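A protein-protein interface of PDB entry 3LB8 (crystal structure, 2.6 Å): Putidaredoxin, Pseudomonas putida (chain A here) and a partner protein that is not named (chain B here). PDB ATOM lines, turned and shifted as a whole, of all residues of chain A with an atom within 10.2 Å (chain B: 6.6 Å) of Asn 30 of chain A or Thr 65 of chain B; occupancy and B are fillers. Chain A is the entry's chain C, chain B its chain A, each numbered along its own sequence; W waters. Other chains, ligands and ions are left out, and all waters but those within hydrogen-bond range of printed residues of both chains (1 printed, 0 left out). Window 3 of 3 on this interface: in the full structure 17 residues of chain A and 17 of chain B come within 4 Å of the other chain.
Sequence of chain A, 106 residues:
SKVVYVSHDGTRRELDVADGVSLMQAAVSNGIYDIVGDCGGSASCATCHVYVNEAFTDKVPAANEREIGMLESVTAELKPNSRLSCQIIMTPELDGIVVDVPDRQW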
ATOM      1  N   SER A   1     -35.034 -26.189   5.978  1.00  0.00           N
ATOM      2  CA  SER A   1     -35.211 -25.171   7.055  1.00  0.00           C
ATOM      3  C   SER A   1     -34.032 -24.199   7.107  1.00  0.00           C
ATOM      4  O   SER A   1     -32.878 -24.588   6.910  1.00  0.00           O
ATOM      5  CB  SER A   1     -35.378 -25.864   8.412  1.00  0.00           C
ATOM      6  OG  SER A   1     -36.530 -26.686   8.426  1.00  0.00           O
ATOM      7  N   VAL A   3     -31.491 -21.273   8.897  1.00  0.00           N
ATOM      8  CA  VAL A   3     -30.829 -20.969  10.152  1.00  0.00           C
ATOM      9  C   VAL A   3     -30.195 -19.599   9.988  1.00  0.00           C
ATOM     10  O   VAL A   3     -29.770 -19.230   8.894  1.00  0.00           O
ATOM     11  CB  VAL A   3     -29.712 -21.983  10.472  1.00  0.00           C
ATOM     12  CG1 VAL A   3     -29.189 -21.757  11.888  1.00  0.00           C
ATOM     13  CG2 VAL A   3     -30.230 -23.396  10.305  1.00  0.00           C
ATOM     14  N   TYR A   5     -27.215 -17.252  11.613  1.00  0.00           N
ATOM     15  CA  TYR A   5     -26.098 -17.147  12.542  1.00  0.00           C
ATOM     16  C   TYR A   5     -25.658 -15.703  12.733  1.00  0.00           C
ATOM     17  O   TYR A   5     -24.927 -15.160  11.902  1.00  0.00           O
ATOM     18  CB  TYR A   5     -24.902 -17.964  12.049  1.00  0.00           C
ATOM     19  CG  TYR A   5     -25.175 -19.435  11.857  1.00  0.00           C
ATOM     20  CD1 TYR A   5     -25.876 -19.894  10.747  1.00  0.00           C
ATOM     21  CD2 TYR A   5     -24.727 -20.368  12.786  1.00  0.00           C
ATOM     22  CE1 TYR A   5     -26.119 -21.245  10.562  1.00  0.00           C
ATOM     23  CE2 TYR A   5     -24.969 -21.723  12.618  1.00  0.00           C
ATOM     24  CZ  TYR A   5     -25.662 -22.157  11.503  1.00  0.00           C
ATOM     25  OH  TYR A   5     -25.899 -23.502  11.330  1.00  0.00           O
ATOM     26  N   ARG A  13     -25.389 -14.188   9.002  1.00  0.00           N
ATOM     27  CA  ARG A  13     -25.364 -15.024   7.808  1.00  0.00           C
ATOM     28  C   ARG A  13     -26.460 -16.084   7.888  1.00  0.00           C
ATOM     29  O   ARG A  13     -26.438 -16.951   8.764  1.00  0.00           O
ATOM     30  CB  ARG A  13     -23.989 -15.692   7.671  1.00  0.00           C
ATOM     31  CG  ARG A  13     -23.899 -16.751   6.578  1.00  0.00           C
ATOM     32  CD  ARG A  13     -24.224 -16.200   5.196  1.00  0.00           C
ATOM     33  NE  ARG A  13     -24.281 -17.257   4.186  1.00  0.00           N
ATOM     34  CZ  ARG A  13     -23.283 -18.101   3.911  1.00  0.00           C
ATOM     35  NH1 ARG A  13     -22.132 -18.028   4.567  1.00  0.00           N
ATOM     36  NH2 ARG A  13     -23.441 -19.021   2.970  1.00  0.00           N
ATOM     37  N   GLU A  14     -27.423 -16.005   6.975  1.00  0.00           N
ATOM     38  CA  GLU A  14     -28.525 -16.957   6.947  1.00  0.00           C
ATOM     39  C   GLU A  14     -28.166 -18.143   6.065  1.00  0.00           C
ATOM     40  O   GLU A  14     -27.452 -17.987   5.073  1.00  0.00           O
ATOM     41  CB  GLU A  14     -29.785 -16.287   6.401  1.00  0.00           C
ATOM     42  CG  GLU A  14     -30.205 -15.030   7.145  1.00  0.00           C
ATOM     43  CD  GLU A  14     -31.449 -14.389   6.546  1.00  0.00           C
ATOM     44  OE1 GLU A  14     -31.862 -13.319   7.041  1.00  0.00           O
ATOM     45  OE2 GLU A  14     -32.011 -14.961   5.583  1.00  0.00           O
ATOM     46  N   LEU A  15     -28.657 -19.327   6.421  1.00  0.00           N
ATOM     47  CA  LEU A  15     -28.363 -20.509   5.622  1.00  0.00           C
ATOM     48  C   LEU A  15     -29.431 -21.576   5.467  1.00  0.00           C
ATOM     49  O   LEU A  15     -30.507 -21.531   6.063  1.00  0.00           O
ATOM     50  CB  LEU A  15     -27.084 -21.190   6.107  1.00  0.00           C
ATOM     51  CG  LEU A  15     -25.783 -20.562   5.615  1.00  0.00           C
ATOM     52  CD1 LEU A  15     -25.357 -19.483   6.574  1.00  0.00           C
ATOM     53  CD2 LEU A  15     -24.709 -21.614   5.527  1.00  0.00           C
ATOM     54  N   ASP A  16     -29.070 -22.549   4.643  1.00  0.00           N
ATOM     55  CA  ASP A  16     -29.896 -23.688   4.281  1.00  0.00           C
ATOM     56  C   ASP A  16     -29.392 -24.971   4.941  1.00  0.00           C
ATOM     57  O   ASP A  16     -28.193 -25.260   4.921  1.00  0.00           O
ATOM     58  CB  ASP A  16     -29.854 -23.823   2.760  1.00  0.00           C
ATOM     59  CG  ASP A  16     -28.504 -23.391   2.181  1.00  0.00           C
ATOM     60  OD1 ASP A  16     -27.503 -24.113   2.384  1.00  0.00           O
ATOM     61  OD2 ASP A  16     -28.437 -22.319   1.539  1.00  0.00           O
ATOM     62  N   VAL A  17     -30.308 -25.741   5.522  1.00  0.00           N
ATOM     63  CA  VAL A  17     -29.950 -26.997   6.182  1.00  0.00           C
ATOM     64  C   VAL A  17     -30.783 -28.152   5.630  1.00  0.00           C
ATOM     65  O   VAL A  17     -32.005 -28.055   5.543  1.00  0.00           O
ATOM     66  CB  VAL A  17     -30.167 -26.910   7.706  1.00  0.00           C
ATOM     67  CG1 VAL A  17     -29.953 -28.276   8.342  1.00  0.00           C
ATOM     68  CG2 VAL A  17     -29.209 -25.895   8.305  1.00  0.00           C
ATOM     69  N   ALA A  18     -30.115 -29.243   5.271  1.00  0.00           N
ATOM     70  CA  ALA A  18     -30.782 -30.421   4.720  1.00  0.00           C
ATOM     71  C   ALA A  18     -31.774 -31.059   5.696  1.00  0.00           C
ATOM     72  O   ALA A  18     -32.440 -32.040   5.358  1.00  0.00           O
ATOM     73  CB  ALA A  18     -29.737 -31.451   4.287  1.00  0.00           C
ATOM     74  N   VAL A  21     -29.356 -32.264  10.101  1.00  0.00           N
ATOM     75  CA  VAL A  21     -27.947 -31.892  10.212  1.00  0.00           C
ATOM     76  C   VAL A  21     -27.811 -30.856  11.316  1.00  0.00           C
ATOM     77  O   VAL A  21     -28.633 -29.949  11.425  1.00  0.00           O
ATOM     78  CB  VAL A  21     -27.430 -31.262   8.904  1.00  0.00           C
ATOM     79  CG1 VAL A  21     -25.980 -30.827   9.071  1.00  0.00           C
ATOM     80  CG2 VAL A  21     -27.576 -32.249   7.757  1.00  0.00           C
ATOM     81  N   SER A  22     -26.770 -30.987  12.129  1.00  0.00           N
ATOM     82  CA  SER A  22     -26.546 -30.063  13.231  1.00  0.00           C
ATOM     83  C   SER A  22     -26.158 -28.693  12.690  1.00  0.00           C
ATOM     84  O   SER A  22     -25.607 -28.586  11.588  1.00  0.00           O
ATOM     85  CB  SER A  22     -25.435 -30.586  14.133  1.00  0.00           C
ATOM     86  OG  SER A  22     -24.198 -30.546  13.447  1.00  0.00           O
ATOM     87  N   LEU A  23     -26.449 -27.655  13.469  1.00  0.00           N
ATOM     88  CA  LEU A  23     -26.124 -26.285  13.087  1.00  0.00           C
ATOM     89  C   LEU A  23     -24.614 -26.077  12.969  1.00  0.00           C
ATOM     90  O   LEU A  23     -24.156 -25.201  12.227  1.00  0.00           O
ATOM     91  CB  LEU A  23     -26.717 -25.309  14.111  1.00  0.00           C
ATOM     92  CG  LEU A  23     -28.126 -24.777  13.820  1.00  0.00           C
ATOM     93  CD1 LEU A  23     -28.950 -25.817  13.075  1.00  0.00           C
ATOM     94  CD2 LEU A  23     -28.791 -24.386  15.131  1.00  0.00           C
ATOM     95  N   MET A  24     -23.848 -26.888  13.701  1.00  0.00           N
ATOM     96  CA  MET A  24     -22.392 -26.818  13.682  1.00  0.00           C
ATOM     97  C   MET A  24     -21.845 -27.285  12.339  1.00  0.00           C
ATOM     98  O   MET A  24     -21.096 -26.561  11.683  1.00  0.00           O
ATOM     99  CB  MET A  24     -21.816 -27.671  14.819  1.00  0.00           C
ATOM    100  CG  MET A  24     -20.293 -27.845  14.809  1.00  0.00           C
ATOM    101  SD  MET A  24     -19.747 -29.311  13.892  1.00  0.00           S
ATOM    102  CE  MET A  24     -18.969 -28.590  12.502  1.00  0.00           C
ATOM    103  N   GLN A  25     -22.227 -28.491  11.922  1.00  0.00           N
ATOM    104  CA  GLN A  25     -21.754 -29.034  10.650  1.00  0.00           C
ATOM    105  C   GLN A  25     -22.028 -28.057   9.513  1.00  0.00           C
ATOM    106  O   GLN A  25     -21.176 -27.837   8.647  1.00  0.00           O
ATOM    107  CB  GLN A  25     -22.434 -30.369  10.336  1.00  0.00           C
ATOM    108  CG  GLN A  25     -21.790 -31.127   9.165  1.00  0.00           C
ATOM    109  CD  GLN A  25     -22.670 -32.259   8.630  1.00  0.00           C
ATOM    110  OE1 GLN A  25     -23.157 -33.099   9.393  1.00  0.00           O
ATOM    111  NE2 GLN A  25     -22.872 -32.281   7.313  1.00  0.00           N
ATOM    112  N   ALA A  26     -23.228 -27.476   9.531  1.00  0.00           N
ATOM    113  CA  ALA A  26     -23.668 -26.520   8.516  1.00  0.00           C
ATOM    114  C   ALA A  26     -22.845 -25.233   8.540  1.00  0.00           C
ATOM    115  O   ALA A  26     -22.402 -24.737   7.499  1.00  0.00           O
ATOM    116  CB  ALA A  26     -25.147 -26.195   8.722  1.00  0.00           C
ATOM    117  N   ALA A  27     -22.650 -24.695   9.738  1.00  0.00           N
ATOM    118  CA  ALA A  27     -21.890 -23.467   9.903  1.00  0.00           C
ATOM    119  C   ALA A  27     -20.445 -23.583   9.416  1.00  0.00           C
ATOM    120  O   ALA A  27     -20.023 -22.806   8.552  1.00  0.00           O
ATOM    121  CB  ALA A  27     -21.915 -23.043  11.360  1.00  0.00           C
ATOM    122  N   VAL A  28     -19.693 -24.547   9.952  1.00  0.00           N
ATOM    123  CA  VAL A  28     -18.290 -24.700   9.564  1.00  0.00           C
ATOM    124  C   VAL A  28     -18.080 -25.095   8.105  1.00  0.00           C
ATOM    125  O   VAL A  28     -17.050 -24.753   7.516  1.00  0.00           O
ATOM    126  CB  VAL A  28     -17.544 -25.733  10.447  1.00  0.00           C
ATOM    127  CG1 VAL A  28     -17.903 -25.535  11.907  1.00  0.00           C
ATOM    128  CG2 VAL A  28     -17.848 -27.132   9.977  1.00  0.00           C
ATOM    129  N   SER A  29     -19.040 -25.807   7.518  1.00  0.00           N
ATOM    130  CA  SER A  29     -18.911 -26.236   6.123  1.00  0.00           C
ATOM    131  C   SER A  29     -19.192 -25.113   5.117  1.00  0.00           C
ATOM    132  O   SER A  29     -18.827 -25.223   3.944  1.00  0.00           O
ATOM    133  CB  SER A  29     -19.845 -27.416   5.843  1.00  0.00           C
ATOM    134  OG  SER A  29     -21.198 -27.017   5.962  1.00  0.00           O
ATOM    135  N   ASN A  30     -19.831 -24.040   5.583  1.00  0.00           N
ATOM    136  CA  ASN A  30     -20.153 -22.899   4.724  1.00  0.00           C
ATOM    137  C   ASN A  30     -19.266 -21.672   4.937  1.00  0.00           C
ATOM    138  O   ASN A  30     -19.489 -20.617   4.335  1.00  0.00           O
ATOM    139  CB  ASN A  30     -21.617 -22.508   4.898  1.00  0.00           C
ATOM    140  CG  ASN A  30     -22.556 -23.541   4.325  1.00  0.00           C
ATOM    141  OD1 ASN A  30     -22.590 -23.757   3.115  1.00  0.00           O
ATOM    142  ND2 ASN A  30     -23.319 -24.195   5.194  1.00  0.00           N
ATOM    143  N   GLY A  31     -18.269 -21.806   5.804  1.00  0.00           N
ATOM    144  CA  GLY A  31     -17.355 -20.706   6.039  1.00  0.00           C
ATOM    145  C   GLY A  31     -17.625 -19.794   7.219  1.00  0.00           C
ATOM    146  O   GLY A  31     -16.974 -18.760   7.346  1.00  0.00           O
ATOM    147  N   ILE A  32     -18.571 -20.146   8.082  1.00  0.00           N
ATOM    148  CA  ILE A  32     -18.847 -19.302   9.239  1.00  0.00           C
ATOM    149  C   ILE A  32     -17.702 -19.455  10.240  1.00  0.00           C
ATOM    150  O   ILE A  32     -17.879 -19.982  11.339  1.00  0.00           O
ATOM    151  CB  ILE A  32     -20.192 -19.676   9.904  1.00  0.00           C
ATOM    152  CG1 ILE A  32     -21.314 -19.590   8.866  1.00  0.00           C
ATOM    153  CG2 ILE A  32     -20.490 -18.727  11.061  1.00  0.00           C
ATOM    154  CD1 ILE A  32     -22.673 -19.956   9.402  1.00  0.00           C
ATOM    155  N   TYR A  33     -16.524 -18.984   9.837  1.00  0.00           N
ATOM    156  CA  TYR A  33     -15.311 -19.048  10.645  1.00  0.00           C
ATOM    157  C   TYR A  33     -15.505 -18.750  12.128  1.00  0.00           C
ATOM    158  O   TYR A  33     -14.775 -19.268  12.973  1.00  0.00           O
ATOM    159  CB  TYR A  33     -14.256 -18.107  10.053  1.00  0.00           C
ATOM    160  CG  TYR A  33     -14.787 -16.762   9.588  1.00  0.00           C
ATOM    161  CD1 TYR A  33     -15.251 -15.811  10.500  1.00  0.00           C
ATOM    162  CD2 TYR A  33     -14.809 -16.435   8.226  1.00  0.00           C
ATOM    163  CE1 TYR A  33     -15.723 -14.565  10.068  1.00  0.00           C
ATOM    164  CE2 TYR A  33     -15.280 -15.196   7.784  1.00  0.00           C
ATOM    165  CZ  TYR A  33     -15.734 -14.266   8.711  1.00  0.00           C
ATOM    166  OH  TYR A  33     -16.186 -13.036   8.277  1.00  0.00           O
ATOM    167  N   ASP A  34     -16.497 -17.920  12.435  1.00  0.00           N
ATOM    168  CA  ASP A  34     -16.812 -17.534  13.807  1.00  0.00           C
ATOM    169  C   ASP A  34     -16.975 -18.756  14.716  1.00  0.00           C
ATOM    170  O   ASP A  34     -16.575 -18.737  15.886  1.00  0.00           O
ATOM    171  CB  ASP A  34     -18.098 -16.711  13.813  1.00  0.00           C
ATOM    172  CG  ASP A  34     -18.139 -15.699  12.687  1.00  0.00           C
ATOM    173  OD1 ASP A  34     -17.316 -14.753  12.706  1.00  0.00           O
ATOM    174  OD2 ASP A  34     -18.987 -15.852  11.776  1.00  0.00           O
ATOM    175  N   ILE A  35     -17.578 -19.813  14.181  1.00  0.00           N
ATOM    176  CA  ILE A  35     -17.770 -21.026  14.961  1.00  0.00           C
ATOM    177  C   ILE A  35     -17.112 -22.246  14.321  1.00  0.00           C
ATOM    178  O   ILE A  35     -17.375 -22.605  13.174  1.00  0.00           O
ATOM    179  CB  ILE A  35     -19.281 -21.312  15.238  1.00  0.00           C
ATOM    180  CG1 ILE A  35     -20.072 -21.435  13.940  1.00  0.00           C
ATOM    181  CG2 ILE A  35     -19.869 -20.187  16.080  1.00  0.00           C
ATOM    182  CD1 ILE A  35     -21.542 -21.720  14.184  1.00  0.00           C
ATOM    183  N   VAL A  36     -16.240 -22.868  15.102  1.00  0.00           N
ATOM    184  CA  VAL A  36     -15.493 -24.037  14.686  1.00  0.00           C
ATOM    185  C   VAL A  36     -16.019 -25.242  15.459  1.00  0.00           C
ATOM    186  O   VAL A  36     -16.554 -25.088  16.550  1.00  0.00           O
ATOM    187  CB  VAL A  36     -14.002 -23.819  14.996  1.00  0.00           C
ATOM    188  CG1 VAL A  36     -13.540 -22.505  14.373  1.00  0.00           C
ATOM    189  CG2 VAL A  36     -13.775 -23.793  16.511  1.00  0.00           C
ATOM    190  N   PHE B  20      -8.679 -21.032   5.030  1.00  0.00           N
ATOM    191  CA  PHE B  20      -9.844 -20.367   5.585  1.00  0.00           C
ATOM    192  C   PHE B  20      -9.536 -19.589   6.854  1.00  0.00           C
ATOM    193  O   PHE B  20     -10.116 -18.527   7.099  1.00  0.00           O
ATOM    194  CB  PHE B  20     -10.953 -21.373   5.855  1.00  0.00           C
ATOM    195  CG  PHE B  20     -11.695 -21.781   4.618  1.00  0.00           C
ATOM    196  CD1 PHE B  20     -11.134 -22.684   3.716  1.00  0.00           C
ATOM    197  CD2 PHE B  20     -12.947 -21.236   4.336  1.00  0.00           C
ATOM    198  CE1 PHE B  20     -11.805 -23.042   2.554  1.00  0.00           C
ATOM    199  CE2 PHE B  20     -13.630 -21.582   3.175  1.00  0.00           C
ATOM    200  CZ  PHE B  20     -13.054 -22.492   2.276  1.00  0.00           C
ATOM    201  N   ILE B  40     -13.033 -33.348  -3.481  1.00  0.00           N
ATOM    202  CA  ILE B  40     -13.274 -32.181  -2.670  1.00  0.00           C
ATOM    203  C   ILE B  40     -12.692 -32.464  -1.289  1.00  0.00           C
ATOM    204  O   ILE B  40     -12.925 -33.522  -0.711  1.00  0.00           O
ATOM    205  CB  ILE B  40     -14.788 -31.885  -2.583  1.00  0.00           C
ATOM    206  CG1 ILE B  40     -15.280 -31.424  -3.948  1.00  0.00           C
ATOM    207  CG2 ILE B  40     -15.068 -30.814  -1.550  1.00  0.00           C
ATOM    208  CD1 ILE B  40     -16.767 -31.162  -3.992  1.00  0.00           C
ATOM    209  N   TYR B  62     -17.367 -33.484   3.481  1.00  0.00           N
ATOM    210  CA  TYR B  62     -16.819 -32.201   3.051  1.00  0.00           C
ATOM    211  C   TYR B  62     -16.332 -31.338   4.197  1.00  0.00           C
ATOM    212  O   TYR B  62     -17.052 -31.113   5.174  1.00  0.00           O
ATOM    213  CB  TYR B  62     -17.858 -31.393   2.280  1.00  0.00           C
ATOM    214  CG  TYR B  62     -18.254 -31.950   0.932  1.00  0.00           C
ATOM    215  CD1 TYR B  62     -19.398 -31.480   0.291  1.00  0.00           C
ATOM    216  CD2 TYR B  62     -17.523 -32.961   0.312  1.00  0.00           C
ATOM    217  CE1 TYR B  62     -19.814 -31.995  -0.919  1.00  0.00           C
ATOM    218  CE2 TYR B  62     -17.935 -33.491  -0.917  1.00  0.00           C
ATOM    219  CZ  TYR B  62     -19.087 -32.997  -1.518  1.00  0.00           C
ATOM    220  OH  TYR B  62     -19.544 -33.503  -2.711  1.00  0.00           O
ATOM    221  N   LEU B  63     -15.105 -30.850   4.077  1.00  0.00           N
ATOM    222  CA  LEU B  63     -14.565 -29.965   5.097  1.00  0.00           C
ATOM    223  C   LEU B  63     -15.332 -28.659   4.960  1.00  0.00           C
ATOM    224  O   LEU B  63     -15.762 -28.074   5.948  1.00  0.00           O
ATOM    225  CB  LEU B  63     -13.073 -29.706   4.868  1.00  0.00           C
ATOM    226  CG  LEU B  63     -12.136 -30.887   5.129  1.00  0.00           C
ATOM    227  CD1 LEU B  63     -10.712 -30.461   4.848  1.00  0.00           C
ATOM    228  CD2 LEU B  63     -12.287 -31.366   6.570  1.00  0.00           C
ATOM    229  N   ARG B  64     -15.493 -28.225   3.713  1.00  0.00           N
ATOM    230  CA  ARG B  64     -16.197 -26.987   3.371  1.00  0.00           C
ATOM    231  C   ARG B  64     -16.981 -27.254   2.102  1.00  0.00           C
ATOM    232  O   ARG B  64     -16.499 -27.968   1.229  1.00  0.00           O
ATOM    233  CB  ARG B  64     -15.199 -25.863   3.074  1.00  0.00           C
ATOM    234  CG  ARG B  64     -14.339 -25.409   4.231  1.00  0.00           C
ATOM    235  CD  ARG B  64     -15.147 -24.607   5.201  1.00  0.00           C
ATOM    236  NE  ARG B  64     -14.294 -24.036   6.228  1.00  0.00           N
ATOM    237  CZ  ARG B  64     -13.697 -24.750   7.172  1.00  0.00           C
ATOM    238  NH1 ARG B  64     -13.865 -26.066   7.220  1.00  0.00           N
ATOM    239  NH2 ARG B  64     -12.924 -24.147   8.065  1.00  0.00           N
ATOM    240  N   THR B  65     -18.173 -26.682   1.986  1.00  0.00           N
ATOM    241  CA  THR B  65     -18.960 -26.881   0.771  1.00  0.00           C
ATOM    242  C   THR B  65     -18.087 -26.369  -0.358  1.00  0.00           C
ATOM    243  O   THR B  65     -17.419 -25.351  -0.212  1.00  0.00           O
ATOM    244  CB  THR B  65     -20.268 -26.073   0.789  1.00  0.00           C
ATOM    245  OG1 THR B  65     -19.965 -24.676   0.889  1.00  0.00           O
ATOM    246  CG2 THR B  65     -21.141 -26.497   1.972  1.00  0.00           C
ATOM    247  N   PRO B  66     -18.080 -27.069  -1.507  1.00  0.00           N
ATOM    248  CA  PRO B  66     -17.260 -26.662  -2.653  1.00  0.00           C
ATOM    249  C   PRO B  66     -17.397 -25.224  -3.144  1.00  0.00           C
ATOM    250  O   PRO B  66     -16.598 -24.789  -3.965  1.00  0.00           O
ATOM    251  CB  PRO B  66     -17.618 -27.695  -3.723  1.00  0.00           C
ATOM    252  CG  PRO B  66     -18.998 -28.113  -3.344  1.00  0.00           C
ATOM    253  CD  PRO B  66     -18.916 -28.230  -1.855  1.00  0.00           C
ATOM    254  N   ASP B  67     -18.378 -24.479  -2.642  1.00  0.00           N
ATOM    255  CA  ASP B  67     -18.541 -23.090  -3.082  1.00  0.00           C
ATOM    256  C   ASP B  67     -18.008 -22.083  -2.070  1.00  0.00           C
ATOM    257  O   ASP B  67     -17.897 -20.892  -2.362  1.00  0.00           O
ATOM    258  CB  ASP B  67     -20.007 -22.784  -3.390  1.00  0.00           C
ATOM    259  CG  ASP B  67     -20.909 -23.046  -2.212  1.00  0.00           C
ATOM    260  OD1 ASP B  67     -20.895 -24.187  -1.694  1.00  0.00           O
ATOM    261  OD2 ASP B  67     -21.637 -22.118  -1.804  1.00  0.00           O
ATOM    262  N   ALA B  68     -17.659 -22.557  -0.879  1.00  0.00           N
ATOM    263  CA  ALA B  68     -17.124 -21.670   0.143  1.00  0.00           C
ATOM    264  C   ALA B  68     -15.731 -21.180  -0.244  1.00  0.00           C
ATOM    265  O   ALA B  68     -15.296 -20.139   0.226  1.00  0.00           O
ATOM    266  CB  ALA B  68     -17.074 -22.383   1.486  1.00  0.00           C
ATOM    267  N   TYR B  69     -15.035 -21.925  -1.100  1.00  0.00           N
ATOM    268  CA  TYR B  69     -13.696 -21.527  -1.517  1.00  0.00           C
ATOM    269  C   TYR B  69     -13.702 -20.251  -2.358  1.00  0.00           C
ATOM    270  O   TYR B  69     -12.883 -19.353  -2.141  1.00  0.00           O
ATOM    271  CB  TYR B  69     -13.001 -22.647  -2.301  1.00  0.00           C
ATOM    272  CG  TYR B  69     -12.784 -23.911  -1.502  1.00  0.00           C
ATOM    273  CD1 TYR B  69     -13.844 -24.769  -1.222  1.00  0.00           C
ATOM    274  CD2 TYR B  69     -11.522 -24.243  -1.010  1.00  0.00           C
ATOM    275  CE1 TYR B  69     -13.660 -25.925  -0.477  1.00  0.00           C
ATOM    276  CE2 TYR B  69     -11.324 -25.402  -0.253  1.00  0.00           C
ATOM    277  CZ  TYR B  69     -12.399 -26.234   0.004  1.00  0.00           C
ATOM    278  OH  TYR B  69     -12.229 -27.384   0.731  1.00  0.00           O
ATOM    279  N   ALA B  71     -16.111 -18.066  -2.424  1.00  0.00           N
ATOM    280  CA  ALA B  71     -16.656 -17.035  -1.547  1.00  0.00           C
ATOM    281  C   ALA B  71     -15.595 -16.347  -0.693  1.00  0.00           C
ATOM    282  O   ALA B  71     -15.706 -15.157  -0.397  1.00  0.00           O
ATOM    283  CB  ALA B  71     -17.714 -17.640  -0.649  1.00  0.00           C
ATOM    284  N   GLN B  72     -14.574 -17.092  -0.286  1.00  0.00           N
ATOM    285  CA  GLN B  72     -13.517 -16.532   0.552  1.00  0.00           C
ATOM    286  C   GLN B  72     -12.323 -16.164  -0.306  1.00  0.00           C
ATOM    287  O   GLN B  72     -11.268 -15.785   0.204  1.00  0.00           O
ATOM    288  CB  GLN B  72     -13.099 -17.545   1.613  1.00  0.00           C
ATOM    289  CG  GLN B  72     -14.257 -18.101   2.409  1.00  0.00           C
ATOM    290  CD  GLN B  72     -14.591 -17.243   3.597  1.00  0.00           C
ATOM    291  OE1 GLN B  72     -14.379 -16.029   3.578  1.00  0.00           O
ATOM    292  NE2 GLN B  72     -15.126 -17.867   4.644  1.00  0.00           N
HETATM  293  O   HOH W   1     -19.765 -31.618   6.605  1.00  0.00           O
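NE of Arg 64 of chain B lies close to O of Val 28 of chain A, 3.1 Å away. The backbone carbonyl oxygen (O) of Ser 29 of chain A is in hydrogen-bond range of the backbone NH (N) of Thr 65 of chain B (2.5 Å). O of Gly 31 of chain A lies within hydrogen-bond range of NE2 of Gln 72 of chain B (3.4 Å).
OD1 of Asp 67 of chain B is in hydrogen-bond range of OG1 of Thr 65 of chain B, 2.8 Å away. The side-chain hydroxyl (OG) of Ser 29 of chain A lies within hydrogen-bond range of the backbone carbonyl oxygen (O) of Gln 25 of chain A (2.8 Å). O of Ala 26 of chain A is in hydrogen-bond range of OG of Ser 29 of chain A (3.0 Å). The backbone carbonyl oxygen (O) of Ala 26 of chain A lies within hydrogen-bond range of the side-chain amide nitrogen (ND2) of Asn 30 of chain A (2.5 Å).
Among the printed residues, pairs that only touch across the chains: Ser 29 of chain A with Arg 64 of chain B, Asn 30 of chain A with Thr 65 of chain B, Ser 29 of chain A with Leu 63 of chain B, Tyr 33 of chain A with Gln 72 of chain B and Val 28 of chain A with Leu 63 of chain B.
Of the printed residues of chain B, Val 28 of chain A touches Leu 63 (3.9 Å) and Arg 64 (3.0 Å). Printed residues of chain B within 4 Å of Ser 29 of chain A: Leu 63 (3.7 Å), Arg 64 (3.2 Å) and Thr 65 (2.5 Å). Asn 30 of chain A touches just one residue of chain B: Thr 65 (3.3 Å). Of the printed residues of chain B, Tyr 33 of chain A touches Gln 72 (3.9 Å). Of the printed residues of chain A, Leu 63 of chain B touches Val 28 (3.9 Å) and Ser 29 (3.7 Å). No residue of chain A comes within 4 Å of Pro 66 of chain B. No residue of chain A comes within 4 Å of Asp 67 of chain B. No residue of chain A comes within 4 Å of Ala 68 of chain B. Of the printed residues of chain A, Gln 72 of chain B touches Gly 31 and Tyr 33.
Among the printed residues, no Asp or Glu carboxylate lies within 4 Å of a Lys or Arg side-chain nitrogen of the other chain.
Water W1 bridges the backbone carbonyl oxygen of Tyr 62 of chain B and the side-chain amide nitrogen of Gln 25 of chain A.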
